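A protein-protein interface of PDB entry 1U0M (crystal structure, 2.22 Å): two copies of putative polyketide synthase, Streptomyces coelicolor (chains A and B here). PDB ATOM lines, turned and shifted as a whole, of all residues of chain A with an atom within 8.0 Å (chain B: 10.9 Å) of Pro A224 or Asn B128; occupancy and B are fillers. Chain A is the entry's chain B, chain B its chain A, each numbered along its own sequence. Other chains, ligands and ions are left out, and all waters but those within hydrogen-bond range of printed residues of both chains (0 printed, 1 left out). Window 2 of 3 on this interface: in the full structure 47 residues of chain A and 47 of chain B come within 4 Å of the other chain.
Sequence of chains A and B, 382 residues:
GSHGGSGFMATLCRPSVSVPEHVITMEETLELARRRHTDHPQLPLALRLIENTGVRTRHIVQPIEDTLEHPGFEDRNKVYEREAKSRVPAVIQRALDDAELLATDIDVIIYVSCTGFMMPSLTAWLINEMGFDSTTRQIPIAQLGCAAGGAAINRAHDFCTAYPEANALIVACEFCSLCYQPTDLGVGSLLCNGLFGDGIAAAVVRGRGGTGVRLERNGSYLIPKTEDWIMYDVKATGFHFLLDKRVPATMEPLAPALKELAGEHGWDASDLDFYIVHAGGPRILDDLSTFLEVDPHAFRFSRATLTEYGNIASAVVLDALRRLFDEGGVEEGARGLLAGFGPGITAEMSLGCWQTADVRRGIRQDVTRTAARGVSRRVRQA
The side-chain amide nitrogen (ND2) of Asn B128 lies close to the backbone NH (N) of Lys A225 (2.6 Å).
OD1 of Asn B128 sits close to OE1 of Glu A227 (3.4 Å).
The backbone NH (N) of Leu A222 sits at hydrogen-bond distance from the backbone carbonyl oxygen (O) of Ser B134, at 3.1 Å.
The side-chain amide oxygen of Gln B138 lies within hydrogen-bond range of the side-chain hydroxyl of Thr B123 (3.0 Å).
O of Ala B124 sits close to OD1 of Asn B128.
The backbone NH (N) of Glu A227 lies close to the backbone carbonyl oxygen (O) of Gly A344 (3.2 Å).
Among the printed residues, pairs that only touch across the chains: Glu A227 with Pro B120 (3.3 Å), Glu A227 with Trp B125 (3.3 Å), Gly A344 with Pro B120 (3.4 Å), Pro A224 with Asn B128 (3.6 Å), Tyr A221 with Ser B134 (3.6 Å), Glu A227 with Glu B129 (3.7 Å), Leu A222 with Asn B128 (3.7 Å), Gly A344 with Ala B124 (3.8 Å) and Leu A222 with Gln B138 (3.95 Å).
Leu A222 touches just these residues of chain B: Asn B128, Ser B134 and Gln B138.
No residue of chain B comes within 4 Å of Ile A223.
Pro A253 touches none of the printed residues of chain B.
Printed residues of chain B within 4 Å of Gly A344: Pro B120 (3.4 Å) and Ala B124 (3.8 Å).
Of chain A, only Leu A222 (3.7 Å), Pro A224 (3.6 Å), Lys A225 (2.6 Å) and Glu A227 (3.3 Å) come within 4 Å of Asn B128.
Of the printed residues of chain A, Glu B129 touches Glu A227.
Phe B132 touches none of the printed residues of chain A.
Of the 12 printed residues of chain A, 6 touch a printed residue of chain B.
Of the 24 printed residues of chain B, 7 touch a printed residue of chain A.
Printed residues of chain B that touch a printed residue of chain A: Pro B120, Ala B124, Trp B125, Asn B128, Glu B129, Ser B134 and Gln B138.
Among the printed residues, 12 pairs touch across the chains.
No position is printed for both chains.
Of the 12 pairs that touch across the chains among the printed residues, none has its exchanged pair printed and touching as well.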
ATOM      1  N   TYR A 221      -8.500  12.452  31.653  1.00  0.00           N
ATOM      2  CA  TYR A 221      -9.786  12.646  30.995  1.00  0.00           C
ATOM      3  C   TYR A 221      -9.680  12.454  29.485  1.00  0.00           C
ATOM      4  O   TYR A 221      -8.676  12.815  28.872  1.00  0.00           O
ATOM      5  CB  TYR A 221     -10.335  14.042  31.314  1.00  0.00           C
ATOM      6  CG  TYR A 221     -11.643  14.349  30.628  1.00  0.00           C
ATOM      7  CD1 TYR A 221     -11.668  14.951  29.369  1.00  0.00           C
ATOM      8  CD2 TYR A 221     -12.861  13.999  31.214  1.00  0.00           C
ATOM      9  CE1 TYR A 221     -12.871  15.196  28.707  1.00  0.00           C
ATOM     10  CE2 TYR A 221     -14.070  14.236  30.562  1.00  0.00           C
ATOM     11  CZ  TYR A 221     -14.067  14.833  29.308  1.00  0.00           C
ATOM     12  OH  TYR A 221     -15.256  15.056  28.649  1.00  0.00           O
ATOM     13  N   LEU A 222     -10.726  11.887  28.893  1.00  0.00           N
ATOM     14  CA  LEU A 222     -10.756  11.623  27.458  1.00  0.00           C
ATOM     15  C   LEU A 222     -11.982  12.259  26.819  1.00  0.00           C
ATOM     16  O   LEU A 222     -13.097  11.810  27.057  1.00  0.00           O
ATOM     17  CB  LEU A 222     -10.766  10.104  27.223  1.00  0.00           C
ATOM     18  CG  LEU A 222     -10.619   9.464  25.831  1.00  0.00           C
ATOM     19  CD1 LEU A 222     -11.877   9.663  25.014  1.00  0.00           C
ATOM     20  CD2 LEU A 222      -9.405  10.051  25.120  1.00  0.00           C
ATOM     21  N   ILE A 223     -11.780  13.303  26.017  1.00  0.00           N
ATOM     22  CA  ILE A 223     -12.899  13.961  25.348  1.00  0.00           C
ATOM     23  C   ILE A 223     -13.514  12.955  24.383  1.00  0.00           C
ATOM     24  O   ILE A 223     -12.840  12.458  23.483  1.00  0.00           O
ATOM     25  CB  ILE A 223     -12.468  15.196  24.525  1.00  0.00           C
ATOM     26  CG1 ILE A 223     -11.603  16.137  25.365  1.00  0.00           C
ATOM     27  CG2 ILE A 223     -13.703  15.942  24.063  1.00  0.00           C
ATOM     28  CD1 ILE A 223     -11.161  17.379  24.619  1.00  0.00           C
ATOM     29  N   PRO A 224     -14.806  12.650  24.559  1.00  0.00           N
ATOM     30  CA  PRO A 224     -15.572  11.704  23.742  1.00  0.00           C
ATOM     31  C   PRO A 224     -15.604  11.982  22.253  1.00  0.00           C
ATOM     32  O   PRO A 224     -15.695  13.131  21.822  1.00  0.00           O
ATOM     33  CB  PRO A 224     -16.970  11.776  24.349  1.00  0.00           C
ATOM     34  CG  PRO A 224     -16.696  12.099  25.781  1.00  0.00           C
ATOM     35  CD  PRO A 224     -15.635  13.165  25.661  1.00  0.00           C
ATOM     36  N   LYS A 225     -15.538  10.903  21.481  1.00  0.00           N
ATOM     37  CA  LYS A 225     -15.597  10.953  20.024  1.00  0.00           C
ATOM     38  C   LYS A 225     -14.681  11.966  19.344  1.00  0.00           C
ATOM     39  O   LYS A 225     -15.130  12.761  18.517  1.00  0.00           O
ATOM     40  CB  LYS A 225     -17.046  11.187  19.607  1.00  0.00           C
ATOM     41  CG  LYS A 225     -17.972  10.105  20.137  1.00  0.00           C
ATOM     42  CD  LYS A 225     -19.378  10.631  20.395  1.00  0.00           C
ATOM     43  CE  LYS A 225     -19.967   9.990  21.648  1.00  0.00           C
ATOM     44  NZ  LYS A 225     -21.292  10.563  22.003  1.00  0.00           N
ATOM     45  N   THR A 226     -13.396  11.920  19.686  1.00  0.00           N
ATOM     46  CA  THR A 226     -12.403  12.816  19.109  1.00  0.00           C
ATOM     47  C   THR A 226     -11.127  12.033  18.781  1.00  0.00           C
ATOM     48  O   THR A 226     -10.039  12.606  18.705  1.00  0.00           O
ATOM     49  CB  THR A 226     -12.059  13.966  20.083  1.00  0.00           C
ATOM     50  OG1 THR A 226     -11.718  13.428  21.364  1.00  0.00           O
ATOM     51  CG2 THR A 226     -13.250  14.904  20.254  1.00  0.00           C
ATOM     52  N   GLU A 227     -11.276  10.725  18.572  1.00  0.00           N
ATOM     53  CA  GLU A 227     -10.141   9.846  18.265  1.00  0.00           C
ATOM     54  C   GLU A 227      -9.286  10.249  17.055  1.00  0.00           C
ATOM     55  O   GLU A 227      -8.059  10.187  17.129  1.00  0.00           O
ATOM     56  CB  GLU A 227     -10.610   8.393  18.068  1.00  0.00           C
ATOM     57  CG  GLU A 227     -11.325   7.774  19.268  1.00  0.00           C
ATOM     58  CD  GLU A 227     -12.841   7.694  19.080  1.00  0.00           C
ATOM     59  OE1 GLU A 227     -13.496   8.748  18.934  1.00  0.00           O
ATOM     60  OE2 GLU A 227     -13.383   6.569  19.074  1.00  0.00           O
ATOM     61  N   ASP A 228      -9.917  10.650  15.950  1.00  0.00           N
ATOM     62  CA  ASP A 228      -9.166  11.035  14.757  1.00  0.00           C
ATOM     63  C   ASP A 228      -8.829  12.520  14.640  1.00  0.00           C
ATOM     64  O   ASP A 228      -8.350  12.973  13.598  1.00  0.00           O
ATOM     65  CB  ASP A 228      -9.902  10.564  13.487  1.00  0.00           C
ATOM     66  CG  ASP A 228     -11.137  11.409  13.150  1.00  0.00           C
ATOM     67  OD1 ASP A 228     -11.850  11.043  12.189  1.00  0.00           O
ATOM     68  OD2 ASP A 228     -11.400  12.432  13.823  1.00  0.00           O
ATOM     69  N   TRP A 229      -9.053  13.265  15.719  1.00  0.00           N
ATOM     70  CA  TRP A 229      -8.793  14.711  15.759  1.00  0.00           C
ATOM     71  C   TRP A 229      -7.319  15.087  15.900  1.00  0.00           C
ATOM     72  O   TRP A 229      -6.890  16.137  15.421  1.00  0.00           O
ATOM     73  CB  TRP A 229      -9.597  15.337  16.896  1.00  0.00           C
ATOM     74  CG  TRP A 229     -11.058  15.362  16.604  1.00  0.00           C
ATOM     75  CD1 TRP A 229     -11.775  14.415  15.929  1.00  0.00           C
ATOM     76  CD2 TRP A 229     -11.982  16.388  16.959  1.00  0.00           C
ATOM     77  NE1 TRP A 229     -13.090  14.792  15.838  1.00  0.00           N
ATOM     78  CE2 TRP A 229     -13.247  16.001  16.463  1.00  0.00           C
ATOM     79  CE3 TRP A 229     -11.867  17.602  17.650  1.00  0.00           C
ATOM     80  CZ2 TRP A 229     -14.394  16.786  16.635  1.00  0.00           C
ATOM     81  CZ3 TRP A 229     -13.009  18.383  17.822  1.00  0.00           C
ATOM     82  CH2 TRP A 229     -14.256  17.969  17.314  1.00  0.00           C
ATOM     83  N   PRO A 253     -15.027  22.021  25.946  1.00  0.00           N
ATOM     84  CA  PRO A 253     -15.395  20.824  26.705  1.00  0.00           C
ATOM     85  C   PRO A 253     -14.327  20.317  27.670  1.00  0.00           C
ATOM     86  O   PRO A 253     -14.624  19.519  28.553  1.00  0.00           O
ATOM     87  CB  PRO A 253     -15.694  19.803  25.610  1.00  0.00           C
ATOM     88  CG  PRO A 253     -16.142  20.648  24.464  1.00  0.00           C
ATOM     89  CD  PRO A 253     -15.118  21.749  24.503  1.00  0.00           C
ATOM     90  N   GLY A 344      -6.387  11.536  21.257  1.00  0.00           N
ATOM     91  CA  GLY A 344      -7.360  10.887  22.113  1.00  0.00           C
ATOM     92  C   GLY A 344      -8.769  11.347  21.784  1.00  0.00           C
ATOM     93  O   GLY A 344      -9.577  10.544  21.329  1.00  0.00           O
ATOM     94  N   ILE A 345      -9.088  12.624  22.006  1.00  0.00           N
ATOM     95  CA  ILE A 345      -8.171  13.616  22.555  1.00  0.00           C
ATOM     96  C   ILE A 345      -7.981  13.339  24.037  1.00  0.00           C
ATOM     97  O   ILE A 345      -8.952  13.236  24.773  1.00  0.00           O
ATOM     98  CB  ILE A 345      -8.737  15.043  22.365  1.00  0.00           C
ATOM     99  CG1 ILE A 345      -8.770  15.389  20.870  1.00  0.00           C
ATOM    100  CG2 ILE A 345      -7.913  16.044  23.145  1.00  0.00           C
ATOM    101  CD1 ILE A 345      -9.122  16.833  20.568  1.00  0.00           C
ATOM    102  N   LYS B  85     -10.314  -3.576  15.611  1.00  0.00           N
ATOM    103  CA  LYS B  85     -11.574  -2.982  16.011  1.00  0.00           C
ATOM    104  C   LYS B  85     -12.691  -4.000  15.979  1.00  0.00           C
ATOM    105  O   LYS B  85     -13.531  -4.016  16.870  1.00  0.00           O
ATOM    106  CB  LYS B  85     -11.899  -1.780  15.132  1.00  0.00           C
ATOM    107  CG  LYS B  85     -11.124  -0.556  15.567  1.00  0.00           C
ATOM    108  CD  LYS B  85     -11.456   0.667  14.743  1.00  0.00           C
ATOM    109  CE  LYS B  85     -10.789   1.900  15.326  1.00  0.00           C
ATOM    110  NZ  LYS B  85     -10.681   2.970  14.312  1.00  0.00           N
ATOM    111  N   PRO B  89     -12.950  -6.040  21.047  1.00  0.00           N
ATOM    112  CA  PRO B  89     -14.151  -5.899  21.887  1.00  0.00           C
ATOM    113  C   PRO B  89     -14.680  -7.181  22.553  1.00  0.00           C
ATOM    114  O   PRO B  89     -14.799  -7.255  23.784  1.00  0.00           O
ATOM    115  CB  PRO B  89     -15.157  -5.291  20.922  1.00  0.00           C
ATOM    116  CG  PRO B  89     -14.295  -4.369  20.127  1.00  0.00           C
ATOM    117  CD  PRO B  89     -13.086  -5.232  19.819  1.00  0.00           C
ATOM    118  N   ILE B  92     -12.346  -8.550  25.284  1.00  0.00           N
ATOM    119  CA  ILE B  92     -12.333  -7.737  26.494  1.00  0.00           C
ATOM    120  C   ILE B  92     -13.556  -8.106  27.329  1.00  0.00           C
ATOM    121  O   ILE B  92     -13.465  -8.300  28.540  1.00  0.00           O
ATOM    122  CB  ILE B  92     -12.363  -6.226  26.155  1.00  0.00           C
ATOM    123  CG1 ILE B  92     -10.973  -5.776  25.690  1.00  0.00           C
ATOM    124  CG2 ILE B  92     -12.809  -5.424  27.363  1.00  0.00           C
ATOM    125  CD1 ILE B  92     -10.906  -4.339  25.224  1.00  0.00           C
ATOM    126  N   ALA B 103     -17.443  -2.471  32.167  1.00  0.00           N
ATOM    127  CA  ALA B 103     -16.450  -1.600  31.564  1.00  0.00           C
ATOM    128  C   ALA B 103     -16.038  -0.526  32.564  1.00  0.00           C
ATOM    129  O   ALA B 103     -14.865  -0.154  32.660  1.00  0.00           O
ATOM    130  CB  ALA B 103     -17.033  -0.949  30.316  1.00  0.00           C
ATOM    131  N   THR B 104     -17.016  -0.066  33.335  1.00  0.00           N
ATOM    132  CA  THR B 104     -16.810   0.998  34.301  1.00  0.00           C
ATOM    133  C   THR B 104     -16.088   0.691  35.610  1.00  0.00           C
ATOM    134  O   THR B 104     -15.957   1.567  36.458  1.00  0.00           O
ATOM    135  CB  THR B 104     -18.147   1.662  34.645  1.00  0.00           C
ATOM    136  OG1 THR B 104     -18.951   1.744  33.461  1.00  0.00           O
ATOM    137  CG2 THR B 104     -17.913   3.064  35.181  1.00  0.00           C
ATOM    138  N   ILE B 109      -6.403   1.114  31.487  1.00  0.00           N
ATOM    139  CA  ILE B 109      -6.301   0.146  30.404  1.00  0.00           C
ATOM    140  C   ILE B 109      -4.828   0.058  30.022  1.00  0.00           C
ATOM    141  O   ILE B 109      -4.130   1.069  29.951  1.00  0.00           O
ATOM    142  CB  ILE B 109      -7.090   0.563  29.155  1.00  0.00           C
ATOM    143  CG1 ILE B 109      -8.589   0.565  29.454  1.00  0.00           C
ATOM    144  CG2 ILE B 109      -6.779  -0.398  28.017  1.00  0.00           C
ATOM    145  CD1 ILE B 109      -9.465   0.791  28.235  1.00  0.00           C
ATOM    146  N   PRO B 120      -3.898   7.997  18.031  1.00  0.00           N
ATOM    147  CA  PRO B 120      -3.842   7.359  19.361  1.00  0.00           C
ATOM    148  C   PRO B 120      -3.905   5.834  19.243  1.00  0.00           C
ATOM    149  O   PRO B 120      -4.266   5.304  18.202  1.00  0.00           O
ATOM    150  CB  PRO B 120      -5.106   7.880  20.072  1.00  0.00           C
ATOM    151  CG  PRO B 120      -5.622   8.979  19.200  1.00  0.00           C
ATOM    152  CD  PRO B 120      -5.225   8.582  17.805  1.00  0.00           C
ATOM    153  N   SER B 121      -3.580   5.134  20.317  1.00  0.00           N
ATOM    154  CA  SER B 121      -3.659   3.685  20.280  1.00  0.00           C
ATOM    155  C   SER B 121      -5.144   3.361  20.358  1.00  0.00           C
ATOM    156  O   SER B 121      -5.978   4.273  20.433  1.00  0.00           O
ATOM    157  CB  SER B 121      -2.924   3.074  21.460  1.00  0.00           C
ATOM    158  OG  SER B 121      -3.558   3.420  22.668  1.00  0.00           O
ATOM    159  N   LEU B 122      -5.473   2.072  20.331  1.00  0.00           N
ATOM    160  CA  LEU B 122      -6.864   1.627  20.377  1.00  0.00           C
ATOM    161  C   LEU B 122      -7.599   2.020  21.662  1.00  0.00           C
ATOM    162  O   LEU B 122      -8.819   2.114  21.666  1.00  0.00           O
ATOM    163  CB  LEU B 122      -6.946   0.100  20.214  1.00  0.00           C
ATOM    164  CG  LEU B 122      -7.675  -0.497  19.001  1.00  0.00           C
ATOM    165  CD1 LEU B 122      -8.243  -1.848  19.414  1.00  0.00           C
ATOM    166  CD2 LEU B 122      -8.805   0.397  18.521  1.00  0.00           C
ATOM    167  N   THR B 123      -6.863   2.240  22.746  1.00  0.00           N
ATOM    168  CA  THR B 123      -7.476   2.602  24.019  1.00  0.00           C
ATOM    169  C   THR B 123      -8.534   3.699  23.910  1.00  0.00           C
ATOM    170  O   THR B 123      -9.615   3.579  24.480  1.00  0.00           O
ATOM    171  CB  THR B 123      -6.433   3.073  25.032  1.00  0.00           C
ATOM    172  OG1 THR B 123      -5.693   4.163  24.468  1.00  0.00           O
ATOM    173  CG2 THR B 123      -5.499   1.925  25.423  1.00  0.00           C
ATOM    174  N   ALA B 124      -8.218   4.771  23.189  1.00  0.00           N
ATOM    175  CA  ALA B 124      -9.156   5.873  23.017  1.00  0.00           C
ATOM    176  C   ALA B 124     -10.460   5.400  22.383  1.00  0.00           C
ATOM    177  O   ALA B 124     -11.546   5.711  22.875  1.00  0.00           O
ATOM    178  CB  ALA B 124      -8.535   6.950  22.161  1.00  0.00           C
ATOM    179  N   TRP B 125     -10.343   4.657  21.286  1.00  0.00           N
ATOM    180  CA  TRP B 125     -11.506   4.142  20.564  1.00  0.00           C
ATOM    181  C   TRP B 125     -12.258   3.130  21.427  1.00  0.00           C
ATOM    182  O   TRP B 125     -13.471   3.005  21.325  1.00  0.00           O
ATOM    183  CB  TRP B 125     -11.058   3.489  19.257  1.00  0.00           C
ATOM    184  CG  TRP B 125     -12.169   2.956  18.397  1.00  0.00           C
ATOM    185  CD1 TRP B 125     -12.923   3.656  17.494  1.00  0.00           C
ATOM    186  CD2 TRP B 125     -12.623   1.598  18.330  1.00  0.00           C
ATOM    187  NE1 TRP B 125     -13.816   2.815  16.868  1.00  0.00           N
ATOM    188  CE2 TRP B 125     -13.651   1.546  17.367  1.00  0.00           C
ATOM    189  CE3 TRP B 125     -12.260   0.419  18.994  1.00  0.00           C
ATOM    190  CZ2 TRP B 125     -14.317   0.360  17.047  1.00  0.00           C
ATOM    191  CZ3 TRP B 125     -12.922  -0.761  18.676  1.00  0.00           C
ATOM    192  CH2 TRP B 125     -13.940  -0.781  17.714  1.00  0.00           C
ATOM    193  N   LEU B 126     -11.531   2.424  22.284  1.00  0.00           N
ATOM    194  CA  LEU B 126     -12.133   1.439  23.173  1.00  0.00           C
ATOM    195  C   LEU B 126     -12.963   2.103  24.265  1.00  0.00           C
ATOM    196  O   LEU B 126     -14.046   1.634  24.595  1.00  0.00           O
ATOM    197  CB  LEU B 126     -11.053   0.566  23.815  1.00  0.00           C
ATOM    198  CG  LEU B 126     -10.451  -0.567  22.984  1.00  0.00           C
ATOM    199  CD1 LEU B 126      -9.290  -1.212  23.753  1.00  0.00           C
ATOM    200  CD2 LEU B 126     -11.531  -1.595  22.683  1.00  0.00           C
ATOM    201  N   ILE B 127     -12.453   3.185  24.835  1.00  0.00           N
ATOM    202  CA  ILE B 127     -13.179   3.895  25.875  1.00  0.00           C
ATOM    203  C   ILE B 127     -14.484   4.425  25.281  1.00  0.00           C
ATOM    204  O   ILE B 127     -15.548   4.312  25.894  1.00  0.00           O
ATOM    205  CB  ILE B 127     -12.318   5.042  26.431  1.00  0.00           C
ATOM    206  CG1 ILE B 127     -11.180   4.439  27.248  1.00  0.00           C
ATOM    207  CG2 ILE B 127     -13.167   6.012  27.259  1.00  0.00           C
ATOM    208  CD1 ILE B 127     -10.044   5.379  27.479  1.00  0.00           C
ATOM    209  N   ASN B 128     -14.396   4.975  24.071  1.00  0.00           N
ATOM    210  CA  ASN B 128     -15.554   5.514  23.370  1.00  0.00           C
ATOM    211  C   ASN B 128     -16.639   4.483  23.074  1.00  0.00           C
ATOM    212  O   ASN B 128     -17.821   4.716  23.333  1.00  0.00           O
ATOM    213  CB  ASN B 128     -15.139   6.125  22.031  1.00  0.00           C
ATOM    214  CG  ASN B 128     -14.833   7.598  22.127  1.00  0.00           C
ATOM    215  OD1 ASN B 128     -13.676   8.002  22.206  1.00  0.00           O
ATOM    216  ND2 ASN B 128     -15.876   8.416  22.121  1.00  0.00           N
ATOM    217  N   GLU B 129     -16.232   3.349  22.512  1.00  0.00           N
ATOM    218  CA  GLU B 129     -17.174   2.309  22.125  1.00  0.00           C
ATOM    219  C   GLU B 129     -17.575   1.344  23.223  1.00  0.00           C
ATOM    220  O   GLU B 129     -18.744   1.002  23.353  1.00  0.00           O
ATOM    221  CB  GLU B 129     -16.612   1.529  20.928  1.00  0.00           C
ATOM    222  CG  GLU B 129     -17.157   1.960  19.557  1.00  0.00           C
ATOM    223  CD  GLU B 129     -17.131   3.468  19.330  1.00  0.00           C
ATOM    224  OE1 GLU B 129     -18.210   4.040  19.063  1.00  0.00           O
ATOM    225  OE2 GLU B 129     -16.041   4.077  19.409  1.00  0.00           O
ATOM    226  N   MET B 130     -16.614   0.898  24.014  1.00  0.00           N
ATOM    227  CA  MET B 130     -16.914  -0.046  25.080  1.00  0.00           C
ATOM    228  C   MET B 130     -17.621   0.622  26.250  1.00  0.00           C
ATOM    229  O   MET B 130     -17.966  -0.030  27.235  1.00  0.00           O
ATOM    230  CB  MET B 130     -15.631  -0.703  25.575  1.00  0.00           C
ATOM    231  CG  MET B 130     -15.715  -2.200  25.689  1.00  0.00           C
ATOM    232  SD  MET B 130     -14.644  -2.948  24.492  1.00  0.00           S
ATOM    233  CE  MET B 130     -15.716  -3.047  23.124  1.00  0.00           C
ATOM    234  N   GLY B 131     -17.823   1.928  26.144  1.00  0.00           N
ATOM    235  CA  GLY B 131     -18.488   2.644  27.211  1.00  0.00           C
ATOM    236  C   GLY B 131     -17.683   2.685  28.492  1.00  0.00           C
ATOM    237  O   GLY B 131     -18.249   2.730  29.577  1.00  0.00           O
ATOM    238  N   PHE B 132     -16.361   2.663  28.381  1.00  0.00           N
ATOM    239  CA  PHE B 132     -15.515   2.722  29.566  1.00  0.00           C
ATOM    240  C   PHE B 132     -15.631   4.078  30.264  1.00  0.00           C
ATOM    241  O   PHE B 132     -16.241   5.017  29.750  1.00  0.00           O
ATOM    242  CB  PHE B 132     -14.054   2.479  29.185  1.00  0.00           C
ATOM    243  CG  PHE B 132     -13.669   1.033  29.136  1.00  0.00           C
ATOM    244  CD1 PHE B 132     -13.226   0.374  30.280  1.00  0.00           C
ATOM    245  CD2 PHE B 132     -13.749   0.323  27.946  1.00  0.00           C
ATOM    246  CE1 PHE B 132     -12.869  -0.965  30.238  1.00  0.00           C
ATOM    247  CE2 PHE B 132     -13.395  -1.017  27.892  1.00  0.00           C
ATOM    248  CZ  PHE B 132     -12.954  -1.663  29.042  1.00  0.00           C
ATOM    249  N   ASP B 133     -15.027   4.159  31.444  1.00  0.00           N
ATOM    250  CA  ASP B 133     -15.013   5.377  32.243  1.00  0.00           C
ATOM    251  C   ASP B 133     -14.310   6.469  31.434  1.00  0.00           C
ATOM    252  O   ASP B 133     -13.182   6.271  30.971  1.00  0.00           O
ATOM    253  CB  ASP B 133     -14.223   5.145  33.539  1.00  0.00           C
ATOM    254  CG  ASP B 133     -14.231   3.682  33.994  1.00  0.00           C
ATOM    255  OD1 ASP B 133     -14.030   2.776  33.148  1.00  0.00           O
ATOM    256  OD2 ASP B 133     -14.417   3.444  35.211  1.00  0.00           O
ATOM    257  N   SER B 134     -14.958   7.618  31.274  1.00  0.00           N
ATOM    258  CA  SER B 134     -14.365   8.723  30.523  1.00  0.00           C
ATOM    259  C   SER B 134     -13.100   9.227  31.235  1.00  0.00           C
ATOM    260  O   SER B 134     -12.458  10.176  30.787  1.00  0.00           O
ATOM    261  CB  SER B 134     -15.384   9.857  30.386  1.00  0.00           C
ATOM    262  OG  SER B 134     -15.070  10.705  29.300  1.00  0.00           O
ATOM    263  N   THR B 135     -12.744   8.558  32.330  1.00  0.00           N
ATOM    264  CA  THR B 135     -11.581   8.906  33.142  1.00  0.00           C
ATOM    265  C   THR B 135     -10.525   7.812  33.165  1.00  0.00           C
ATOM    266  O   THR B 135      -9.477   7.974  33.788  1.00  0.00           O
ATOM    267  CB  THR B 135     -11.992   9.189  34.609  1.00  0.00           C
ATOM    268  OG1 THR B 135     -12.711   8.064  35.136  1.00  0.00           O
ATOM    269  CG2 THR B 135     -12.874  10.408  34.681  1.00  0.00           C
ATOM    270  N   THR B 136     -10.804   6.697  32.494  1.00  0.00           N
ATOM    271  CA  THR B 136      -9.876   5.566  32.448  1.00  0.00           C
ATOM    272  C   THR B 136      -8.522   5.996  31.907  1.00  0.00           C
ATOM    273  O   THR B 136      -8.445   6.668  30.887  1.00  0.00           O
ATOM    274  CB  THR B 136     -10.399   4.437  31.541  1.00  0.00           C
ATOM    275  OG1 THR B 136     -11.814   4.310  31.699  1.00  0.00           O
ATOM    276  CG2 THR B 136      -9.732   3.117  31.904  1.00  0.00           C
ATOM    277  N   GLN B 138      -5.028   5.515  30.053  1.00  0.00           N
ATOM    278  CA  GLN B 138      -4.554   4.689  28.952  1.00  0.00           C
ATOM    279  C   GLN B 138      -3.046   4.482  29.101  1.00  0.00           C
ATOM    280  O   GLN B 138      -2.305   5.425  29.372  1.00  0.00           O
ATOM    281  CB  GLN B 138      -4.848   5.384  27.620  1.00  0.00           C
ATOM    282  CG  GLN B 138      -6.286   5.829  27.470  1.00  0.00           C
ATOM    283  CD  GLN B 138      -6.420   7.026  26.563  1.00  0.00           C
ATOM    284  OE1 GLN B 138      -6.375   6.907  25.341  1.00  0.00           O
ATOM    285  NE2 GLN B 138      -6.569   8.202  27.164  1.00  0.00           N
